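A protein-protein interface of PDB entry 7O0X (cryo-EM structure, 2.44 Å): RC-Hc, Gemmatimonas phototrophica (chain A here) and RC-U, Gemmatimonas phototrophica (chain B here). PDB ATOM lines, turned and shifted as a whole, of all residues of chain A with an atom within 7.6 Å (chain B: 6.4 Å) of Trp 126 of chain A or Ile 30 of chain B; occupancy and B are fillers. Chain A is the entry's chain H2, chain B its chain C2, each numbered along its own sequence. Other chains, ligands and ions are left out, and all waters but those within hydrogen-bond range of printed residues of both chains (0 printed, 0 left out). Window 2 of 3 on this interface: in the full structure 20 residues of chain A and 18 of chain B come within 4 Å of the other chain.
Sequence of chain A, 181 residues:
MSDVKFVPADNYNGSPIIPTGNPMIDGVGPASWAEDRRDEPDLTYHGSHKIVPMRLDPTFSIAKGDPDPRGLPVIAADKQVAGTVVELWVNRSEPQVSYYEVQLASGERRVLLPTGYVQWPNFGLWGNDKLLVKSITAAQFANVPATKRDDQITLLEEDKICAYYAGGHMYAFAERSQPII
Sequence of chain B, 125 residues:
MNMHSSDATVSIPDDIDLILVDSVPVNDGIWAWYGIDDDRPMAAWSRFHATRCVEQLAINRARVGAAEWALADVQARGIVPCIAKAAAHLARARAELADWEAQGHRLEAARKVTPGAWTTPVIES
The backbone carbonyl oxygen (O) of Val 26 of chain B lies within hydrogen-bond range of the side-chain amide nitrogen (ND2) of Asn 128 of chain A (2.6 Å). The backbone NH of Gly 127 of chain A sits at hydrogen-bond distance from the backbone carbonyl oxygen of Asn 27 of chain B. The backbone NH (N) of Ile 30 of chain B lies within hydrogen-bond range of the backbone carbonyl oxygen (O) of Leu 125 of chain A, 3.2 Å away.
The side-chain amide nitrogen (ND2) of Asn 122 of chain A sits at hydrogen-bond distance from the backbone carbonyl oxygen (O) of Trp 126 of chain A. The side-chain amide nitrogen (ND2) of Asn 128 of chain A lies within hydrogen-bond range of the backbone carbonyl oxygen (O) of Gly 124 of chain A.
CA of Gly 29 of chain B touches O of Leu 125 of chain A, at 3.3 Å. Trp 126 of chain A touches Asn 27 of chain B. CB of Trp 126 of chain A touches O of Asp 28 of chain B, at 3.4 Å. Trp 126 of chain A touches Ile 30 of chain B. Trp 126 of chain A touches Trp 31 of chain B.
Trp 126 of chain A touches four residues of chain B. Printed residues of chain B within 4 Å of Gly 127 of chain A: Asn 27. Of the printed residues of chain A, Asp 28 of chain B touches Trp 126. Gly 29 of chain B touches one residue of chain A. Of the printed residues of chain A, Ile 30 of chain B touches Leu 125 (3.2 Å) and Trp 126 (3.7 Å).
Hydrophobic or aromatic side chains of chain B within 4 Å of the printed part of chain A: Ile 30 and Trp 31. Of the 10 printed residues of chain A, 4 touch a printed residue of chain B. Among the printed residues, 8 pairs touch across the chains.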
ATOM      1  N   TRP A 120     -19.284  -7.686  24.146  1.00  0.00           N
ATOM      2  CA  TRP A 120     -18.983  -8.784  25.052  1.00  0.00           C
ATOM      3  C   TRP A 120     -18.334  -8.270  26.341  1.00  0.00           C
ATOM      4  O   TRP A 120     -17.692  -7.218  26.340  1.00  0.00           O
ATOM      5  CB  TRP A 120     -18.082  -9.793  24.352  1.00  0.00           C
ATOM      6  CG  TRP A 120     -18.802 -10.498  23.238  1.00  0.00           C
ATOM      7  CD1 TRP A 120     -18.968 -10.049  21.961  1.00  0.00           C
ATOM      8  CD2 TRP A 120     -19.472 -11.765  23.304  1.00  0.00           C
ATOM      9  NE1 TRP A 120     -19.689 -10.955  21.228  1.00  0.00           N
ATOM     10  CE2 TRP A 120     -20.010 -12.019  22.028  1.00  0.00           C
ATOM     11  CE3 TRP A 120     -19.662 -12.709  24.317  1.00  0.00           C
ATOM     12  CZ2 TRP A 120     -20.727 -13.179  21.737  1.00  0.00           C
ATOM     13  CZ3 TRP A 120     -20.372 -13.860  24.025  1.00  0.00           C
ATOM     14  CH2 TRP A 120     -20.896 -14.084  22.747  1.00  0.00           C
ATOM     15  N   PRO A 121     -18.493  -9.005  27.452  1.00  0.00           N
ATOM     16  CA  PRO A 121     -18.249  -8.402  28.780  1.00  0.00           C
ATOM     17  C   PRO A 121     -16.872  -7.786  28.990  1.00  0.00           C
ATOM     18  O   PRO A 121     -16.781  -6.641  29.450  1.00  0.00           O
ATOM     19  CB  PRO A 121     -18.485  -9.585  29.729  1.00  0.00           C
ATOM     20  CG  PRO A 121     -19.513 -10.390  29.036  1.00  0.00           C
ATOM     21  CD  PRO A 121     -19.115 -10.333  27.579  1.00  0.00           C
ATOM     22  N   ASN A 122     -15.797  -8.504  28.678  1.00  0.00           N
ATOM     23  CA  ASN A 122     -14.462  -7.996  28.974  1.00  0.00           C
ATOM     24  C   ASN A 122     -13.663  -7.751  27.702  1.00  0.00           C
ATOM     25  O   ASN A 122     -12.520  -8.204  27.578  1.00  0.00           O
ATOM     26  CB  ASN A 122     -13.719  -8.961  29.900  1.00  0.00           C
ATOM     27  CG  ASN A 122     -14.493  -9.262  31.165  1.00  0.00           C
ATOM     28  OD1 ASN A 122     -14.665  -8.394  32.021  1.00  0.00           O
ATOM     29  ND2 ASN A 122     -14.980 -10.490  31.285  1.00  0.00           N
ATOM     30  N   PHE A 123     -14.276  -7.052  26.747  1.00  0.00           N
ATOM     31  CA  PHE A 123     -13.839  -7.024  25.351  1.00  0.00           C
ATOM     32  C   PHE A 123     -13.694  -8.427  24.762  1.00  0.00           C
ATOM     33  O   PHE A 123     -12.936  -8.632  23.810  1.00  0.00           O
ATOM     34  CB  PHE A 123     -12.543  -6.218  25.196  1.00  0.00           C
ATOM     35  CG  PHE A 123     -12.561  -4.903  25.933  1.00  0.00           C
ATOM     36  CD1 PHE A 123     -13.552  -3.968  25.678  1.00  0.00           C
ATOM     37  CD2 PHE A 123     -11.594  -4.604  26.878  1.00  0.00           C
ATOM     38  CE1 PHE A 123     -13.579  -2.763  26.353  1.00  0.00           C
ATOM     39  CE2 PHE A 123     -11.615  -3.397  27.556  1.00  0.00           C
ATOM     40  CZ  PHE A 123     -12.610  -2.477  27.292  1.00  0.00           C
ATOM     41  N   GLY A 124     -14.416  -9.399  25.318  1.00  0.00           N
ATOM     42  CA  GLY A 124     -14.349 -10.777  24.879  1.00  0.00           C
ATOM     43  C   GLY A 124     -13.168 -11.577  25.382  1.00  0.00           C
ATOM     44  O   GLY A 124     -13.009 -12.733  24.969  1.00  0.00           O
ATOM     45  N   LEU A 125     -12.332 -11.009  26.253  1.00  0.00           N
ATOM     46  CA  LEU A 125     -11.123 -11.693  26.697  1.00  0.00           C
ATOM     47  C   LEU A 125     -11.389 -12.785  27.727  1.00  0.00           C
ATOM     48  O   LEU A 125     -10.551 -13.679  27.886  1.00  0.00           O
ATOM     49  CB  LEU A 125     -10.133 -10.677  27.267  1.00  0.00           C
ATOM     50  CG  LEU A 125      -9.565  -9.684  26.253  1.00  0.00           C
ATOM     51  CD1 LEU A 125      -8.759  -8.608  26.954  1.00  0.00           C
ATOM     52  CD2 LEU A 125      -8.712 -10.406  25.222  1.00  0.00           C
ATOM     53  N   TRP A 126     -12.525 -12.738  28.415  1.00  0.00           N
ATOM     54  CA  TRP A 126     -12.985 -13.819  29.284  1.00  0.00           C
ATOM     55  C   TRP A 126     -14.431 -13.518  29.666  1.00  0.00           C
ATOM     56  O   TRP A 126     -14.980 -12.471  29.311  1.00  0.00           O
ATOM     57  CB  TRP A 126     -12.098 -13.997  30.522  1.00  0.00           C
ATOM     58  CG  TRP A 126     -12.241 -12.937  31.578  1.00  0.00           C
ATOM     59  CD1 TRP A 126     -13.049 -12.984  32.676  1.00  0.00           C
ATOM     60  CD2 TRP A 126     -11.516 -11.703  31.667  1.00  0.00           C
ATOM     61  NE1 TRP A 126     -12.895 -11.844  33.425  1.00  0.00           N
ATOM     62  CE2 TRP A 126     -11.958 -11.043  32.830  1.00  0.00           C
ATOM     63  CE3 TRP A 126     -10.548 -11.087  30.870  1.00  0.00           C
ATOM     64  CZ2 TRP A 126     -11.464  -9.799  33.217  1.00  0.00           C
ATOM     65  CZ3 TRP A 126     -10.058  -9.850  31.255  1.00  0.00           C
ATOM     66  CH2 TRP A 126     -10.517  -9.221  32.418  1.00  0.00           C
ATOM     67  N   GLY A 127     -15.044 -14.448  30.393  1.00  0.00           N
ATOM     68  CA  GLY A 127     -16.439 -14.322  30.770  1.00  0.00           C
ATOM     69  C   GLY A 127     -17.338 -14.880  29.687  1.00  0.00           C
ATOM     70  O   GLY A 127     -17.792 -16.024  29.780  1.00  0.00           O
ATOM     71  N   ASN A 128     -17.582 -14.078  28.648  1.00  0.00           N
ATOM     72  CA  ASN A 128     -18.268 -14.521  27.430  1.00  0.00           C
ATOM     73  C   ASN A 128     -19.583 -15.249  27.715  1.00  0.00           C
ATOM     74  O   ASN A 128     -19.927 -16.234  27.060  1.00  0.00           O
ATOM     75  CB  ASN A 128     -17.334 -15.371  26.571  1.00  0.00           C
ATOM     76  CG  ASN A 128     -16.129 -14.585  26.088  1.00  0.00           C
ATOM     77  OD1 ASN A 128     -16.255 -13.435  25.668  1.00  0.00           O
ATOM     78  ND2 ASN A 128     -14.955 -15.197  26.153  1.00  0.00           N
ATOM     79  N   ASP A 129     -20.323 -14.758  28.709  1.00  0.00           N
ATOM     80  CA  ASP A 129     -21.484 -15.460  29.238  1.00  0.00           C
ATOM     81  C   ASP A 129     -22.733 -14.588  29.266  1.00  0.00           C
ATOM     82  O   ASP A 129     -23.769 -15.031  29.772  1.00  0.00           O
ATOM     83  CB  ASP A 129     -21.191 -16.004  30.646  1.00  0.00           C
ATOM     84  CG  ASP A 129     -20.815 -14.914  31.632  1.00  0.00           C
ATOM     85  OD1 ASP A 129     -20.383 -13.829  31.192  1.00  0.00           O
ATOM     86  OD2 ASP A 129     -20.942 -15.149  32.853  1.00  0.00           O
ATOM     87  N   PRO B  25      -9.846 -21.021  25.476  1.00  0.00           N
ATOM     88  CA  PRO B  25     -11.013 -21.406  26.276  1.00  0.00           C
ATOM     89  C   PRO B  25     -11.966 -20.232  26.470  1.00  0.00           C
ATOM     90  O   PRO B  25     -11.544 -19.188  26.956  1.00  0.00           O
ATOM     91  CB  PRO B  25     -10.398 -21.846  27.612  1.00  0.00           C
ATOM     92  CG  PRO B  25      -8.986 -22.202  27.280  1.00  0.00           C
ATOM     93  CD  PRO B  25      -8.588 -21.235  26.205  1.00  0.00           C
ATOM     94  N   VAL B  26     -13.232 -20.403  26.086  1.00  0.00           N
ATOM     95  CA  VAL B  26     -14.129 -19.257  25.956  1.00  0.00           C
ATOM     96  C   VAL B  26     -14.407 -18.604  27.311  1.00  0.00           C
ATOM     97  O   VAL B  26     -14.487 -17.374  27.409  1.00  0.00           O
ATOM     98  CB  VAL B  26     -15.428 -19.662  25.232  1.00  0.00           C
ATOM     99  CG1 VAL B  26     -15.111 -20.264  23.874  1.00  0.00           C
ATOM    100  CG2 VAL B  26     -16.243 -20.642  26.061  1.00  0.00           C
ATOM    101  N   ASN B  27     -14.557 -19.401  28.373  1.00  0.00           N
ATOM    102  CA  ASN B  27     -15.022 -18.845  29.642  1.00  0.00           C
ATOM    103  C   ASN B  27     -13.904 -18.175  30.439  1.00  0.00           C
ATOM    104  O   ASN B  27     -14.044 -17.022  30.861  1.00  0.00           O
ATOM    105  CB  ASN B  27     -15.685 -19.939  30.480  1.00  0.00           C
ATOM    106  CG  ASN B  27     -16.955 -20.472  29.845  1.00  0.00           C
ATOM    107  OD1 ASN B  27     -17.693 -19.735  29.194  1.00  0.00           O
ATOM    108  ND2 ASN B  27     -17.220 -21.759  30.039  1.00  0.00           N
ATOM    109  N   ASP B  28     -12.798 -18.882  30.670  1.00  0.00           N
ATOM    110  CA  ASP B  28     -11.677 -18.311  31.411  1.00  0.00           C
ATOM    111  C   ASP B  28     -10.727 -17.499  30.540  1.00  0.00           C
ATOM    112  O   ASP B  28     -10.008 -16.643  31.067  1.00  0.00           O
ATOM    113  CB  ASP B  28     -10.915 -19.421  32.133  1.00  0.00           C
ATOM    114  CG  ASP B  28     -11.802 -20.214  33.073  1.00  0.00           C
ATOM    115  OD1 ASP B  28     -12.131 -19.693  34.160  1.00  0.00           O
ATOM    116  OD2 ASP B  28     -12.186 -21.349  32.721  1.00  0.00           O
ATOM    117  N   GLY B  29     -10.722 -17.735  29.237  1.00  0.00           N
ATOM    118  CA  GLY B  29      -9.989 -16.899  28.299  1.00  0.00           C
ATOM    119  C   GLY B  29      -8.508 -16.768  28.607  1.00  0.00           C
ATOM    120  O   GLY B  29      -7.783 -17.764  28.720  1.00  0.00           O
ATOM    121  N   ILE B  30      -8.046 -15.522  28.747  1.00  0.00           N
ATOM    122  CA  ILE B  30      -6.648 -15.247  29.085  1.00  0.00           C
ATOM    123  C   ILE B  30      -6.235 -15.842  30.426  1.00  0.00           C
ATOM    124  O   ILE B  30      -5.063 -16.187  30.619  1.00  0.00           O
ATOM    125  CB  ILE B  30      -6.388 -13.728  29.041  1.00  0.00           C
ATOM    126  CG1 ILE B  30      -7.161 -13.007  30.148  1.00  0.00           C
ATOM    127  CG2 ILE B  30      -6.745 -13.167  27.674  1.00  0.00           C
ATOM    128  CD1 ILE B  30      -6.893 -11.519  30.205  1.00  0.00           C
ATOM    129  N   TRP B  31      -7.165 -15.978  31.369  1.00  0.00           N
ATOM    130  CA  TRP B  31      -6.797 -16.475  32.691  1.00  0.00           C
ATOM    131  C   TRP B  31      -6.430 -17.954  32.680  1.00  0.00           C
ATOM    132  O   TRP B  31      -5.810 -18.430  33.636  1.00  0.00           O
ATOM    133  CB  TRP B  31      -7.920 -16.206  33.692  1.00  0.00           C
ATOM    134  CG  TRP B  31      -8.208 -14.743  33.839  1.00  0.00           C
ATOM    135  CD1 TRP B  31      -9.190 -14.039  33.212  1.00  0.00           C
ATOM    136  CD2 TRP B  31      -7.465 -13.791  34.614  1.00  0.00           C
ATOM    137  NE1 TRP B  31      -9.130 -12.716  33.574  1.00  0.00           N
ATOM    138  CE2 TRP B  31      -8.076 -12.536  34.430  1.00  0.00           C
ATOM    139  CE3 TRP B  31      -6.351 -13.881  35.454  1.00  0.00           C
ATOM    140  CZ2 TRP B  31      -7.613 -11.381  35.055  1.00  0.00           C
ATOM    141  CZ3 TRP B  31      -5.892 -12.732  36.075  1.00  0.00           C
ATOM    142  CH2 TRP B  31      -6.522 -11.499  35.871  1.00  0.00           C
ATOM    143  N   ALA B  32      -6.799 -18.688  31.628  1.00  0.00           N
ATOM    144  CA  ALA B  32      -6.294 -20.047  31.453  1.00  0.00           C
ATOM    145  C   ALA B  32      -4.774 -20.101  31.320  1.00  0.00           C
ATOM    146  O   ALA B  32      -4.168 -21.122  31.661  1.00  0.00           O
ATOM    147  CB  ALA B  32      -6.953 -20.693  30.235  1.00  0.00           C
ATOM    148  N   TRP B  33      -4.132 -19.027  30.844  1.00  0.00           N
ATOM    149  CA  TRP B  33      -2.669 -19.021  30.809  1.00  0.00           C
ATOM    150  C   TRP B  33      -2.068 -19.128  32.205  1.00  0.00           C
ATOM    151  O   TRP B  33      -0.997 -19.721  32.376  1.00  0.00           O
ATOM    152  CB  TRP B  33      -2.139 -17.749  30.139  1.00  0.00           C
ATOM    153  CG  TRP B  33      -2.634 -17.427  28.753  1.00  0.00           C
ATOM    154  CD1 TRP B  33      -3.107 -16.221  28.325  1.00  0.00           C
ATOM    155  CD2 TRP B  33      -2.594 -18.273  27.593  1.00  0.00           C
ATOM    156  NE1 TRP B  33      -3.421 -16.280  26.991  1.00  0.00           N
ATOM    157  CE2 TRP B  33      -3.111 -17.525  26.516  1.00  0.00           C
ATOM    158  CE3 TRP B  33      -2.197 -19.595  27.367  1.00  0.00           C
ATOM    159  CZ2 TRP B  33      -3.239 -18.054  25.233  1.00  0.00           C
ATOM    160  CZ3 TRP B  33      -2.328 -20.118  26.089  1.00  0.00           C
ATOM    161  CH2 TRP B  33      -2.844 -19.348  25.041  1.00  0.00           C
ATOM    162  N   TYR B  34      -2.737 -18.567  33.208  1.00  0.00           N
ATOM    163  CA  TYR B  34      -2.301 -18.623  34.596  1.00  0.00           C
ATOM    164  C   TYR B  34      -2.932 -19.777  35.361  1.00  0.00           C
ATOM    165  O   TYR B  34      -2.822 -19.831  36.590  1.00  0.00           O
ATOM    166  CB  TYR B  34      -2.590 -17.287  35.280  1.00  0.00           C
ATOM    167  CG  TYR B  34      -2.208 -16.117  34.405  1.00  0.00           C
ATOM    168  CD1 TYR B  34      -0.889 -15.923  34.016  1.00  0.00           C
ATOM    169  CD2 TYR B  34      -3.165 -15.234  33.934  1.00  0.00           C
ATOM    170  CE1 TYR B  34      -0.532 -14.861  33.209  1.00  0.00           C
ATOM    171  CE2 TYR B  34      -2.820 -14.174  33.120  1.00  0.00           C
ATOM    172  CZ  TYR B  34      -1.501 -13.992  32.762  1.00  0.00           C
ATOM    173  OH  TYR B  34      -1.155 -12.941  31.945  1.00  0.00           O
ATOM    174  N   GLY B  35      -3.594 -20.690  34.659  1.00  0.00           N
ATOM    175  CA  GLY B  35      -4.141 -21.895  35.242  1.00  0.00           C
ATOM    176  C   GLY B  35      -5.419 -21.742  36.028  1.00  0.00           C
ATOM    177  O   GLY B  35      -5.779 -22.665  36.766  1.00  0.00           O
